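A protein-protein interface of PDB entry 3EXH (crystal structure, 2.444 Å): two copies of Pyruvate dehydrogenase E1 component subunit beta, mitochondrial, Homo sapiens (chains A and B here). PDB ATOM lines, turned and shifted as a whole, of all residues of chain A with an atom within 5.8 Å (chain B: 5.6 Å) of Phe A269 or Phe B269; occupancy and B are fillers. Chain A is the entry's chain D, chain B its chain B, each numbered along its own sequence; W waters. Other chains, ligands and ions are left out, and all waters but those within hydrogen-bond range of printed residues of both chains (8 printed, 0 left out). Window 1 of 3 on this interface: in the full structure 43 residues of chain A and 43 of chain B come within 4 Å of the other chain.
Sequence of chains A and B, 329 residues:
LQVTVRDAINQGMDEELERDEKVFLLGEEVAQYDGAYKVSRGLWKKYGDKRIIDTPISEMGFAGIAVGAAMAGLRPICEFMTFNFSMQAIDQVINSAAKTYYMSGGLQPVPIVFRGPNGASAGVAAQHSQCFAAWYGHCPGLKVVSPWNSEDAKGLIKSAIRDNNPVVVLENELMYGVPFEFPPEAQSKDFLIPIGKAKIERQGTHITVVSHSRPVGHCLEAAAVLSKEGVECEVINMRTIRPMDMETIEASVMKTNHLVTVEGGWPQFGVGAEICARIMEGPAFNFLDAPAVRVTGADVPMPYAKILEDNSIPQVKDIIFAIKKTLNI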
ATOM      1  N   ALA A 133      24.384 -14.172 -29.195  1.00  0.00           N
ATOM      2  CA  ALA A 133      23.656 -14.592 -28.012  1.00  0.00           C
ATOM      3  C   ALA A 133      24.256 -15.854 -27.345  1.00  0.00           C
ATOM      4  O   ALA A 133      24.504 -15.862 -26.132  1.00  0.00           O
ATOM      5  CB  ALA A 133      22.167 -14.823 -28.370  1.00  0.00           C
ATOM      6  N   ALA A 134      24.469 -16.918 -28.104  1.00  0.00           N
ATOM      7  CA  ALA A 134      24.987 -18.130 -27.485  1.00  0.00           C
ATOM      8  C   ALA A 134      26.442 -17.939 -26.945  1.00  0.00           C
ATOM      9  O   ALA A 134      26.822 -18.579 -25.959  1.00  0.00           O
ATOM     10  CB  ALA A 134      24.888 -19.331 -28.426  1.00  0.00           C
ATOM     11  N   GLY A 137      25.931 -15.734 -23.768  1.00  0.00           N
ATOM     12  CA  GLY A 137      25.037 -16.385 -22.827  1.00  0.00           C
ATOM     13  C   GLY A 137      25.790 -17.432 -22.014  1.00  0.00           C
ATOM     14  O   GLY A 137      25.366 -17.797 -20.919  1.00  0.00           O
ATOM     15  N   HIS A 138      26.910 -17.914 -22.561  1.00  0.00           N
ATOM     16  CA  HIS A 138      27.723 -19.035 -22.046  1.00  0.00           C
ATOM     17  C   HIS A 138      28.464 -18.600 -20.800  1.00  0.00           C
ATOM     18  O   HIS A 138      28.793 -19.451 -20.016  1.00  0.00           O
ATOM     19  CB  HIS A 138      28.715 -19.398 -23.135  1.00  0.00           C
ATOM     20  CG  HIS A 138      29.571 -20.608 -22.885  1.00  0.00           C
ATOM     21  ND1 HIS A 138      29.061 -21.860 -22.590  1.00  0.00           N
ATOM     22  CD2 HIS A 138      30.914 -20.788 -23.049  1.00  0.00           C
ATOM     23  CE1 HIS A 138      30.053 -22.735 -22.523  1.00  0.00           C
ATOM     24  NE2 HIS A 138      31.188 -22.112 -22.794  1.00  0.00           N
ATOM     25  N   ILE A 241      18.580 -13.853 -22.425  1.00  0.00           N
ATOM     26  CA  ILE A 241      19.428 -14.981 -22.777  1.00  0.00           C
ATOM     27  C   ILE A 241      20.177 -15.548 -21.534  1.00  0.00           C
ATOM     28  O   ILE A 241      20.202 -16.751 -21.322  1.00  0.00           O
ATOM     29  CB  ILE A 241      20.469 -14.605 -23.864  1.00  0.00           C
ATOM     30  CG1 ILE A 241      19.763 -14.052 -25.121  1.00  0.00           C
ATOM     31  CG2 ILE A 241      21.318 -15.809 -24.226  1.00  0.00           C
ATOM     32  CD1 ILE A 241      18.618 -15.004 -25.665  1.00  0.00           C
ATOM     33  N   ARG A 242      20.763 -14.687 -20.708  1.00  0.00           N
ATOM     34  CA  ARG A 242      21.314 -15.151 -19.442  1.00  0.00           C
ATOM     35  C   ARG A 242      21.033 -14.181 -18.266  1.00  0.00           C
ATOM     36  O   ARG A 242      21.422 -13.033 -18.293  1.00  0.00           O
ATOM     37  CB  ARG A 242      22.819 -15.410 -19.580  1.00  0.00           C
ATOM     38  CG  ARG A 242      23.475 -15.987 -18.299  1.00  0.00           C
ATOM     39  CD  ARG A 242      25.023 -15.977 -18.309  1.00  0.00           C
ATOM     40  NE  ARG A 242      25.493 -16.744 -17.156  1.00  0.00           N
ATOM     41  CZ  ARG A 242      25.833 -18.034 -17.190  1.00  0.00           C
ATOM     42  NH1 ARG A 242      25.798 -18.741 -18.320  1.00  0.00           N
ATOM     43  NH2 ARG A 242      26.228 -18.630 -16.071  1.00  0.00           N
ATOM     44  N   MET A 244      18.242 -17.204 -18.424  1.00  0.00           N
ATOM     45  CA  MET A 244      17.040 -17.395 -19.201  1.00  0.00           C
ATOM     46  C   MET A 244      15.948 -17.867 -18.267  1.00  0.00           C
ATOM     47  O   MET A 244      16.245 -18.501 -17.274  1.00  0.00           O
ATOM     48  CB  MET A 244      17.263 -18.337 -20.381  1.00  0.00           C
ATOM     49  CG  MET A 244      17.378 -19.819 -20.025  1.00  0.00           C
ATOM     50  SD  MET A 244      17.376 -20.858 -21.526  1.00  0.00           S
ATOM     51  CE  MET A 244      18.863 -20.260 -22.379  1.00  0.00           C
ATOM     52  N   TRP A 266      23.491 -19.387 -35.643  1.00  0.00           N
ATOM     53  CA  TRP A 266      23.948 -20.691 -36.093  1.00  0.00           C
ATOM     54  C   TRP A 266      23.407 -21.762 -35.170  1.00  0.00           C
ATOM     55  O   TRP A 266      23.201 -21.523 -33.989  1.00  0.00           O
ATOM     56  CB  TRP A 266      25.495 -20.728 -36.142  1.00  0.00           C
ATOM     57  CG  TRP A 266      26.085 -19.830 -37.217  1.00  0.00           C
ATOM     58  CD1 TRP A 266      25.583 -19.614 -38.493  1.00  0.00           C
ATOM     59  CD2 TRP A 266      27.267 -19.000 -37.119  1.00  0.00           C
ATOM     60  NE1 TRP A 266      26.401 -18.747 -39.186  1.00  0.00           N
ATOM     61  CE2 TRP A 266      27.424 -18.343 -38.359  1.00  0.00           C
ATOM     62  CE3 TRP A 266      28.209 -18.768 -36.117  1.00  0.00           C
ATOM     63  CZ2 TRP A 266      28.467 -17.478 -38.602  1.00  0.00           C
ATOM     64  CZ3 TRP A 266      29.259 -17.899 -36.376  1.00  0.00           C
ATOM     65  CH2 TRP A 266      29.375 -17.257 -37.586  1.00  0.00           C
ATOM     66  N   PRO A 267      23.143 -22.939 -35.701  1.00  0.00           N
ATOM     67  CA  PRO A 267      22.534 -24.063 -34.950  1.00  0.00           C
ATOM     68  C   PRO A 267      23.383 -24.754 -33.860  1.00  0.00           C
ATOM     69  O   PRO A 267      22.862 -25.094 -32.791  1.00  0.00           O
ATOM     70  CB  PRO A 267      22.211 -25.093 -36.035  1.00  0.00           C
ATOM     71  CG  PRO A 267      23.063 -24.783 -37.119  1.00  0.00           C
ATOM     72  CD  PRO A 267      23.341 -23.275 -37.106  1.00  0.00           C
ATOM     73  N   GLN A 268      24.654 -25.027 -34.116  1.00  0.00           N
ATOM     74  CA  GLN A 268      25.393 -25.834 -33.171  1.00  0.00           C
ATOM     75  C   GLN A 268      25.828 -25.080 -31.924  1.00  0.00           C
ATOM     76  O   GLN A 268      26.457 -24.028 -32.028  1.00  0.00           O
ATOM     77  CB  GLN A 268      26.547 -26.484 -33.905  1.00  0.00           C
ATOM     78  CG  GLN A 268      25.998 -27.309 -35.090  1.00  0.00           C
ATOM     79  CD  GLN A 268      27.049 -28.164 -35.744  1.00  0.00           C
ATOM     80  OE1 GLN A 268      27.657 -29.030 -35.108  1.00  0.00           O
ATOM     81  NE2 GLN A 268      27.251 -27.945 -37.039  1.00  0.00           N
ATOM     82  N   PHE A 269      25.476 -25.583 -30.741  1.00  0.00           N
ATOM     83  CA  PHE A 269      25.877 -24.907 -29.538  1.00  0.00           C
ATOM     84  C   PHE A 269      25.165 -23.570 -29.437  1.00  0.00           C
ATOM     85  O   PHE A 269      25.685 -22.650 -28.781  1.00  0.00           O
ATOM     86  CB  PHE A 269      27.407 -24.698 -29.494  1.00  0.00           C
ATOM     87  CG  PHE A 269      28.177 -25.947 -29.843  1.00  0.00           C
ATOM     88  CD1 PHE A 269      28.191 -27.054 -28.973  1.00  0.00           C
ATOM     89  CD2 PHE A 269      28.793 -26.070 -31.080  1.00  0.00           C
ATOM     90  CE1 PHE A 269      28.862 -28.230 -29.345  1.00  0.00           C
ATOM     91  CE2 PHE A 269      29.493 -27.239 -31.442  1.00  0.00           C
ATOM     92  CZ  PHE A 269      29.519 -28.322 -30.573  1.00  0.00           C
ATOM     93  N   GLY A 270      23.954 -23.460 -30.023  1.00  0.00           N
ATOM     94  CA  GLY A 270      23.245 -22.178 -30.027  1.00  0.00           C
ATOM     95  C   GLY A 270      22.174 -22.088 -28.953  1.00  0.00           C
ATOM     96  O   GLY A 270      22.088 -22.968 -28.074  1.00  0.00           O
ATOM     97  N   VAL A 271      21.315 -21.065 -29.035  1.00  0.00           N
ATOM     98  CA  VAL A 271      20.386 -20.813 -27.962  1.00  0.00           C
ATOM     99  C   VAL A 271      19.386 -21.942 -27.823  1.00  0.00           C
ATOM    100  O   VAL A 271      19.050 -22.331 -26.714  1.00  0.00           O
ATOM    101  CB  VAL A 271      19.732 -19.460 -28.128  1.00  0.00           C
ATOM    102  CG1 VAL A 271      18.714 -19.248 -27.005  1.00  0.00           C
ATOM    103  CG2 VAL A 271      20.833 -18.390 -28.165  1.00  0.00           C
ATOM    104  N   GLY A 272      18.901 -22.452 -28.954  1.00  0.00           N
ATOM    105  CA  GLY A 272      17.933 -23.552 -28.959  1.00  0.00           C
ATOM    106  C   GLY A 272      18.493 -24.838 -28.345  1.00  0.00           C
ATOM    107  O   GLY A 272      17.749 -25.607 -27.728  1.00  0.00           O
ATOM    108  N   ALA A 273      19.798 -25.084 -28.509  1.00  0.00           N
ATOM    109  CA  ALA A 273      20.433 -26.280 -27.905  1.00  0.00           C
ATOM    110  C   ALA A 273      20.288 -26.231 -26.423  1.00  0.00           C
ATOM    111  O   ALA A 273      20.008 -27.262 -25.773  1.00  0.00           O
ATOM    112  CB  ALA A 273      21.908 -26.370 -28.221  1.00  0.00           C
ATOM    113  N   GLU A 274      20.536 -25.047 -25.857  1.00  0.00           N
ATOM    114  CA  GLU A 274      20.439 -24.947 -24.412  1.00  0.00           C
ATOM    115  C   GLU A 274      18.977 -25.170 -24.020  1.00  0.00           C
ATOM    116  O   GLU A 274      18.716 -25.913 -23.079  1.00  0.00           O
ATOM    117  CB  GLU A 274      20.968 -23.609 -23.867  1.00  0.00           C
ATOM    118  CG  GLU A 274      20.913 -23.502 -22.299  1.00  0.00           C
ATOM    119  CD  GLU A 274      21.774 -24.568 -21.503  1.00  0.00           C
ATOM    120  OE1 GLU A 274      22.735 -25.165 -22.054  1.00  0.00           O
ATOM    121  OE2 GLU A 274      21.484 -24.806 -20.293  1.00  0.00           O
ATOM    122  N   ARG A 294      14.524 -27.554 -33.268  1.00  0.00           N
ATOM    123  CA  ARG A 294      15.054 -26.219 -33.428  1.00  0.00           C
ATOM    124  C   ARG A 294      14.989 -25.680 -34.836  1.00  0.00           C
ATOM    125  O   ARG A 294      15.353 -26.361 -35.779  1.00  0.00           O
ATOM    126  CB  ARG A 294      16.482 -26.180 -32.954  1.00  0.00           C
ATOM    127  CG  ARG A 294      16.676 -26.562 -31.490  1.00  0.00           C
ATOM    128  CD  ARG A 294      18.201 -26.635 -31.281  1.00  0.00           C
ATOM    129  NE  ARG A 294      18.821 -27.747 -32.017  1.00  0.00           N
ATOM    130  CZ  ARG A 294      20.131 -27.927 -32.129  1.00  0.00           C
ATOM    131  NH1 ARG A 294      20.977 -27.046 -31.601  1.00  0.00           N
ATOM    132  NH2 ARG A 294      20.600 -29.000 -32.749  1.00  0.00           N
ATOM    133  N   ALA B 133      35.577 -24.866 -26.259  1.00  0.00           N
ATOM    134  CA  ALA B 133      35.140 -25.844 -27.268  1.00  0.00           C
ATOM    135  C   ALA B 133      33.832 -25.458 -27.928  1.00  0.00           C
ATOM    136  O   ALA B 133      33.751 -25.493 -29.157  1.00  0.00           O
ATOM    137  CB  ALA B 133      35.036 -27.263 -26.686  1.00  0.00           C
ATOM    138  N   ALA B 134      32.822 -25.112 -27.129  1.00  0.00           N
ATOM    139  CA  ALA B 134      31.495 -24.712 -27.648  1.00  0.00           C
ATOM    140  C   ALA B 134      31.597 -23.379 -28.436  1.00  0.00           C
ATOM    141  O   ALA B 134      31.016 -23.213 -29.508  1.00  0.00           O
ATOM    142  CB  ALA B 134      30.436 -24.597 -26.463  1.00  0.00           C
ATOM    143  N   GLY B 137      33.350 -24.497 -31.752  1.00  0.00           N
ATOM    144  CA  GLY B 137      32.446 -25.448 -32.410  1.00  0.00           C
ATOM    145  C   GLY B 137      31.214 -24.795 -33.050  1.00  0.00           C
ATOM    146  O   GLY B 137      30.575 -25.363 -33.919  1.00  0.00           O
ATOM    147  N   HIS B 138      30.866 -23.608 -32.572  1.00  0.00           N
ATOM    148  CA  HIS B 138      29.730 -22.860 -33.024  1.00  0.00           C
ATOM    149  C   HIS B 138      29.885 -22.367 -34.478  1.00  0.00           C
ATOM    150  O   HIS B 138      28.875 -22.163 -35.147  1.00  0.00           O
ATOM    151  CB  HIS B 138      29.592 -21.638 -32.106  1.00  0.00           C
ATOM    152  CG  HIS B 138      28.324 -20.866 -32.302  1.00  0.00           C
ATOM    153  ND1 HIS B 138      27.072 -21.460 -32.263  1.00  0.00           N
ATOM    154  CD2 HIS B 138      28.109 -19.540 -32.504  1.00  0.00           C
ATOM    155  CE1 HIS B 138      26.146 -20.542 -32.464  1.00  0.00           C
ATOM    156  NE2 HIS B 138      26.740 -19.371 -32.607  1.00  0.00           N
ATOM    157  N   ILE B 241      35.047 -31.852 -32.171  1.00  0.00           N
ATOM    158  CA  ILE B 241      33.963 -31.033 -31.676  1.00  0.00           C
ATOM    159  C   ILE B 241      33.176 -30.461 -32.875  1.00  0.00           C
ATOM    160  O   ILE B 241      31.951 -30.358 -32.802  1.00  0.00           O
ATOM    161  CB  ILE B 241      34.491 -29.892 -30.842  1.00  0.00           C
ATOM    162  CG1 ILE B 241      35.291 -30.459 -29.645  1.00  0.00           C
ATOM    163  CG2 ILE B 241      33.345 -28.914 -30.489  1.00  0.00           C
ATOM    164  CD1 ILE B 241      34.505 -31.110 -28.603  1.00  0.00           C
ATOM    165  N   ARG B 242      33.867 -30.059 -33.951  1.00  0.00           N
ATOM    166  CA  ARG B 242      33.173 -29.630 -35.190  1.00  0.00           C
ATOM    167  C   ARG B 242      33.923 -30.110 -36.443  1.00  0.00           C
ATOM    168  O   ARG B 242      35.079 -29.685 -36.642  1.00  0.00           O
ATOM    169  CB  ARG B 242      33.036 -28.097 -35.318  1.00  0.00           C
ATOM    170  CG  ARG B 242      32.167 -27.734 -36.533  1.00  0.00           C
ATOM    171  CD  ARG B 242      32.117 -26.275 -36.850  1.00  0.00           C
ATOM    172  NE  ARG B 242      31.153 -25.986 -37.905  1.00  0.00           N
ATOM    173  CZ  ARG B 242      29.887 -25.564 -37.710  1.00  0.00           C
ATOM    174  NH1 ARG B 242      29.408 -25.306 -36.478  1.00  0.00           N
ATOM    175  NH2 ARG B 242      29.088 -25.393 -38.775  1.00  0.00           N
ATOM    176  N   MET B 244      30.984 -32.790 -35.301  1.00  0.00           N
ATOM    177  CA  MET B 244      30.977 -33.938 -34.408  1.00  0.00           C
ATOM    178  C   MET B 244      30.356 -35.173 -35.062  1.00  0.00           C
ATOM    179  O   MET B 244      29.587 -35.087 -36.022  1.00  0.00           O
ATOM    180  CB  MET B 244      30.258 -33.611 -33.095  1.00  0.00           C
ATOM    181  CG  MET B 244      28.826 -33.370 -33.284  1.00  0.00           C
ATOM    182  SD  MET B 244      28.002 -33.185 -31.670  1.00  0.00           S
ATOM    183  CE  MET B 244      28.663 -31.539 -31.288  1.00  0.00           C
ATOM    184  N   TRP B 266      31.796 -24.757 -19.074  1.00  0.00           N
ATOM    185  CA  TRP B 266      30.573 -24.213 -18.487  1.00  0.00           C
ATOM    186  C   TRP B 266      29.310 -24.825 -19.123  1.00  0.00           C
ATOM    187  O   TRP B 266      29.287 -25.142 -20.314  1.00  0.00           O
ATOM    188  CB  TRP B 266      30.516 -22.707 -18.696  1.00  0.00           C
ATOM    189  CG  TRP B 266      31.557 -21.924 -17.942  1.00  0.00           C
ATOM    190  CD1 TRP B 266      32.010 -22.156 -16.655  1.00  0.00           C
ATOM    191  CD2 TRP B 266      32.266 -20.747 -18.424  1.00  0.00           C
ATOM    192  NE1 TRP B 266      32.965 -21.192 -16.326  1.00  0.00           N
ATOM    193  CE2 TRP B 266      33.123 -20.317 -17.387  1.00  0.00           C
ATOM    194  CE3 TRP B 266      32.269 -20.039 -19.630  1.00  0.00           C
ATOM    195  CZ2 TRP B 266      33.949 -19.203 -17.522  1.00  0.00           C
ATOM    196  CZ3 TRP B 266      33.109 -18.881 -19.747  1.00  0.00           C
ATOM    197  CH2 TRP B 266      33.943 -18.514 -18.710  1.00  0.00           C
ATOM    198  N   PRO B 267      28.246 -24.942 -18.349  1.00  0.00           N
ATOM    199  CA  PRO B 267      27.148 -25.734 -18.857  1.00  0.00           C
ATOM    200  C   PRO B 267      26.264 -25.083 -19.954  1.00  0.00           C
ATOM    201  O   PRO B 267      25.837 -25.776 -20.925  1.00  0.00           O
ATOM    202  CB  PRO B 267      26.323 -26.040 -17.587  1.00  0.00           C
ATOM    203  CG  PRO B 267      26.621 -24.860 -16.637  1.00  0.00           C
ATOM    204  CD  PRO B 267      28.110 -24.609 -16.919  1.00  0.00           C
ATOM    205  N   GLN B 268      25.945 -23.804 -19.826  1.00  0.00           N
ATOM    206  CA  GLN B 268      24.899 -23.271 -20.687  1.00  0.00           C
ATOM    207  C   GLN B 268      25.446 -23.048 -22.096  1.00  0.00           C
ATOM    208  O   GLN B 268      26.531 -22.463 -22.249  1.00  0.00           O
ATOM    209  CB  GLN B 268      24.250 -21.998 -20.089  1.00  0.00           C
ATOM    210  CG  GLN B 268      24.008 -22.076 -18.566  1.00  0.00           C
ATOM    211  CD  GLN B 268      22.973 -21.099 -18.062  1.00  0.00           C
ATOM    212  OE1 GLN B 268      21.869 -20.990 -18.643  1.00  0.00           O
ATOM    213  NE2 GLN B 268      23.296 -20.398 -16.941  1.00  0.00           N
ATOM    214  N   PHE B 269      24.741 -23.538 -23.128  1.00  0.00           N
ATOM    215  CA  PHE B 269      25.202 -23.397 -24.504  1.00  0.00           C
ATOM    216  C   PHE B 269      26.572 -24.090 -24.708  1.00  0.00           C
ATOM    217  O   PHE B 269      27.343 -23.733 -25.625  1.00  0.00           O
ATOM    218  CB  PHE B 269      25.336 -21.909 -24.889  1.00  0.00           C
ATOM    219  CG  PHE B 269      24.196 -21.057 -24.412  1.00  0.00           C
ATOM    220  CD1 PHE B 269      22.999 -21.023 -25.107  1.00  0.00           C
ATOM    221  CD2 PHE B 269      24.315 -20.319 -23.239  1.00  0.00           C
ATOM    222  CE1 PHE B 269      21.925 -20.226 -24.639  1.00  0.00           C
ATOM    223  CE2 PHE B 269      23.267 -19.537 -22.755  1.00  0.00           C
ATOM    224  CZ  PHE B 269      22.067 -19.472 -23.444  1.00  0.00           C
ATOM    225  N   GLY B 270      26.857 -25.078 -23.871  1.00  0.00           N
ATOM    226  CA  GLY B 270      28.102 -25.849 -23.973  1.00  0.00           C
ATOM    227  C   GLY B 270      27.957 -27.048 -24.872  1.00  0.00           C
ATOM    228  O   GLY B 270      26.980 -27.164 -25.623  1.00  0.00           O
ATOM    229  N   VAL B 271      28.943 -27.932 -24.844  1.00  0.00           N
ATOM    230  CA  VAL B 271      29.011 -29.012 -25.827  1.00  0.00           C
ATOM    231  C   VAL B 271      27.909 -30.038 -25.597  1.00  0.00           C
ATOM    232  O   VAL B 271      27.323 -30.582 -26.574  1.00  0.00           O
ATOM    233  CB  VAL B 271      30.420 -29.691 -25.765  1.00  0.00           C
ATOM    234  CG1 VAL B 271      30.487 -31.025 -26.511  1.00  0.00           C
ATOM    235  CG2 VAL B 271      31.528 -28.671 -26.161  1.00  0.00           C
ATOM    236  N   GLY B 272      27.630 -30.333 -24.331  1.00  0.00           N
ATOM    237  CA  GLY B 272      26.600 -31.340 -23.992  1.00  0.00           C
ATOM    238  C   GLY B 272      25.215 -30.884 -24.413  1.00  0.00           C
ATOM    239  O   GLY B 272      24.326 -31.687 -24.759  1.00  0.00           O
ATOM    240  N   ALA B 273      25.004 -29.572 -24.371  1.00  0.00           N
ATOM    241  CA  ALA B 273      23.727 -29.040 -24.771  1.00  0.00           C
ATOM    242  C   ALA B 273      23.569 -29.469 -26.216  1.00  0.00           C
ATOM    243  O   ALA B 273      22.500 -29.909 -26.622  1.00  0.00           O
ATOM    244  CB  ALA B 273      23.685 -27.447 -24.632  1.00  0.00           C
ATOM    245  N   GLU B 274      24.609 -29.316 -27.017  1.00  0.00           N
ATOM    246  CA  GLU B 274      24.410 -29.603 -28.436  1.00  0.00           C
ATOM    247  C   GLU B 274      24.165 -31.111 -28.672  1.00  0.00           C
ATOM    248  O   GLU B 274      23.417 -31.504 -29.547  1.00  0.00           O
ATOM    249  CB  GLU B 274      25.586 -29.085 -29.311  1.00  0.00           C
ATOM    250  CG  GLU B 274      25.502 -29.485 -30.765  1.00  0.00           C
ATOM    251  CD  GLU B 274      24.301 -28.861 -31.505  1.00  0.00           C
ATOM    252  OE1 GLU B 274      23.720 -27.840 -31.052  1.00  0.00           O
ATOM    253  OE2 GLU B 274      23.930 -29.390 -32.568  1.00  0.00           O
ATOM    254  N   ARG B 294      23.450 -33.968 -18.527  1.00  0.00           N
ATOM    255  CA  ARG B 294      24.774 -33.382 -18.723  1.00  0.00           C
ATOM    256  C   ARG B 294      25.623 -33.291 -17.448  1.00  0.00           C
ATOM    257  O   ARG B 294      25.168 -32.792 -16.444  1.00  0.00           O
ATOM    258  CB  ARG B 294      24.607 -31.999 -19.286  1.00  0.00           C
ATOM    259  CG  ARG B 294      23.989 -32.004 -20.645  1.00  0.00           C
ATOM    260  CD  ARG B 294      23.860 -30.590 -21.137  1.00  0.00           C
ATOM    261  NE  ARG B 294      22.922 -29.813 -20.316  1.00  0.00           N
ATOM    262  CZ  ARG B 294      22.755 -28.489 -20.404  1.00  0.00           C
ATOM    263  NH1 ARG B 294      23.463 -27.758 -21.256  1.00  0.00           N
ATOM    264  NH2 ARG B 294      21.864 -27.896 -19.652  1.00  0.00           N
HETATM  265  O   HOH W   1      26.823 -24.089 -35.977  1.00  0.00           O
HETATM  266  O   HOH W   2      20.827 -18.357 -19.123  1.00  0.00           O
HETATM  267  O   HOH W   3      25.439 -17.461 -34.363  1.00  0.00           O
HETATM  268  O   HOH W   4      33.174 -22.578 -25.151  1.00  0.00           O
HETATM  269  O   HOH W   5      26.546 -17.090 -30.587  1.00  0.00           O
HETATM  270  O   HOH W   6      28.625 -20.924 -26.033  1.00  0.00           O
HETATM  271  O   HOH W   7      33.283 -23.015 -21.094  1.00  0.00           O
HETATM  272  O   HOH W   8      27.025 -21.265 -18.570  1.00  0.00           O
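Water W2 lies within hydrogen-bond range of the backbone carbonyl oxygen (O) of Ile A241 (2.8 Å), the side-chain amide oxygen (OE1) of Gln B268 (2.9 Å) and the backbone NH (N) of Met A244 (2.9 Å).
Water W8 lies within hydrogen-bond range of the guanidinium group of Arg A242 (2.8 Å), the backbone carbonyl oxygen of His A138 (2.9 Å) and the backbone NH of Gln B268 (3.0 Å).
Water W7 lies within hydrogen-bond range of a ring nitrogen (NE2) of His A138 and the backbone NH of Trp B266.
Water W3 bridges a ring nitrogen (NE2) of His B138 (2.9 Å) and the backbone NH of Trp A266 (3.0 Å).
Water W6 lies within hydrogen-bond range of O of Ala A134 and O of Phe B269.
Water W5 bridges NE2 of His B138 (3.1 Å) and N of Ala A134 (3.2 Å).
Met A244 touches Phe B269, and with the chains exchanged Phe A269 touches Met B244.
Ala A273 touches its own counterpart, Ala B273.
Ala A273 touches Glu B274, and with the chains exchanged Glu A274 touches Ala B273.
Glu A274 touches Arg B294, and with the chains exchanged Arg A294 touches Glu B274.
Of the 33 pairs that touch across the chains among the printed residues, 32 have their exchanged pair printed and touching as well.
The backbone carbonyl oxygen (O) of Gly B137 is in hydrogen-bond range of the guanidinium group (NH1) of Arg B242, at 2.8 Å.
The backbone carbonyl oxygen of His B138 is in hydrogen-bond range of the guanidinium group of Arg B242 (3.5 Å).
O of Pro B267 is in hydrogen-bond range of NH1 of Arg B294, at 3.1 Å.
O of Gly A137 sits at hydrogen-bond distance from NH1 of Arg A242, 2.8 Å away.
The backbone carbonyl oxygen (O) of Pro A267 is in hydrogen-bond range of the guanidinium group (NH1) of Arg A294 (3.0 Å).
Among the printed residues, merely in contact across the chains: Glu A274 with Gln B268 (3.2 Å), Gly A137 with Phe B269 (3.3 Å), Phe A269 with Gly B137 (3.3 Å), His A138 with Trp B266 (3.4 Å), Gln A268 with Glu B274 (3.4 Å), Phe A269 with Met B244 (3.4 Å), Trp A266 with His B138 (3.5 Å), Met A244 with Phe B269 (3.5 Å), Phe A269 with His B138 (3.5 Å), Phe A269 with Gly B270 (3.6 Å), Glu A274 with Ala B273 (3.6 Å), His A138 with Phe B269 (3.6 Å), Phe A269 with Val B271 (3.6 Å), Gly A270 with Phe B269 (3.7 Å), Ala A273 with Glu B274 (3.7 Å), Val A271 with Phe B269 (3.7 Å), Phe A269 with Phe B269 (3.7 Å), Ala A273 with Ala B273 (3.7 Å), Ala A134 with Phe B269 (3.8 Å), Ile A241 with Phe B269 (3.8 Å), Phe A269 with Ile B241 (3.9 Å), Phe A269 with Ala B134 (3.9 Å) and His A138 with Gly B270 (3.95 Å).
Printed residues of chain A within 4 Å of Ile B241: Phe A269.
Of the printed residues of chain A, Gly B270 touches His A138 (3.95 Å) and Phe A269 (3.6 Å).
Of the printed residues of chain A, Pro B267 touches Glu A274 (3.4 Å).
Ala B133 touches none of the printed residues of chain A.
The nearest residue of chain A that does not touch Phe B269 is Ala A133 (5.1 Å).
Of the 17 printed residues of chain A, 15 touch a printed residue of chain B.
Printed residues of chain A that touch a printed residue of chain B: Ala A134, Gly A137, His A138, Ile A241, Arg A242, Met A244, Trp A266, Pro A267, Gln A268, Phe A269, Gly A270, Val A271, Ala A273, Glu A274 and Arg A294.
Hydrophobic or aromatic side chains of chain A within 4 Å of the printed part of chain B: His A138, Ile A241, Met A244, Trp A266, Phe A269 and Ala A273.
Of the 17 printed residues of chain B, 15 touch a printed residue of chain A.
Among the printed residues, 33 pairs touch across the chains.
Among the printed residues, Asp or Glu carboxylates within 4 Å of a Lys or Arg side-chain nitrogen of the other chain: Glu A274 with Arg B294 (2.8 Å) and Arg A294 with Glu B274 (2.9 Å).
ND1 of His B138 is in hydrogen-bond range of O of Gln A268 (2.7 Å).
NH1 of Arg B242 lies close to NE2 of Gln A268 (3.5 Å).
The backbone carbonyl oxygen of Gln B268 sits at hydrogen-bond distance from a ring nitrogen (ND1) of His A138, at 2.6 Å.
The side-chain amide nitrogen (NE2) of Gln B268 lies close to the guanidinium group (NH1) of Arg A242 (3.3 Å).
The backbone NH (N) of Phe B269 lies within hydrogen-bond range of the side-chain carboxylate (OE1) of Glu A274 (2.8 Å).
OE1 of Glu B274 sits at hydrogen-bond distance from N of Phe A269, at 2.9 Å.
The guanidinium group (NH1) of Arg A294 lies within salt-bridge range of the side-chain carboxylate (OE1) of Glu B274.
The guanidinium group (NH1) of Arg B294 is in salt-bridge range of the side-chain carboxylate (OE1) of Glu A274 (2.8 Å).
O of Pro A267 lies close to OE1 of Glu B274 (3.4 Å).
The backbone carbonyl oxygen of Pro B267 lies close to the side-chain carboxylate of Glu A274 (3.4 Å).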
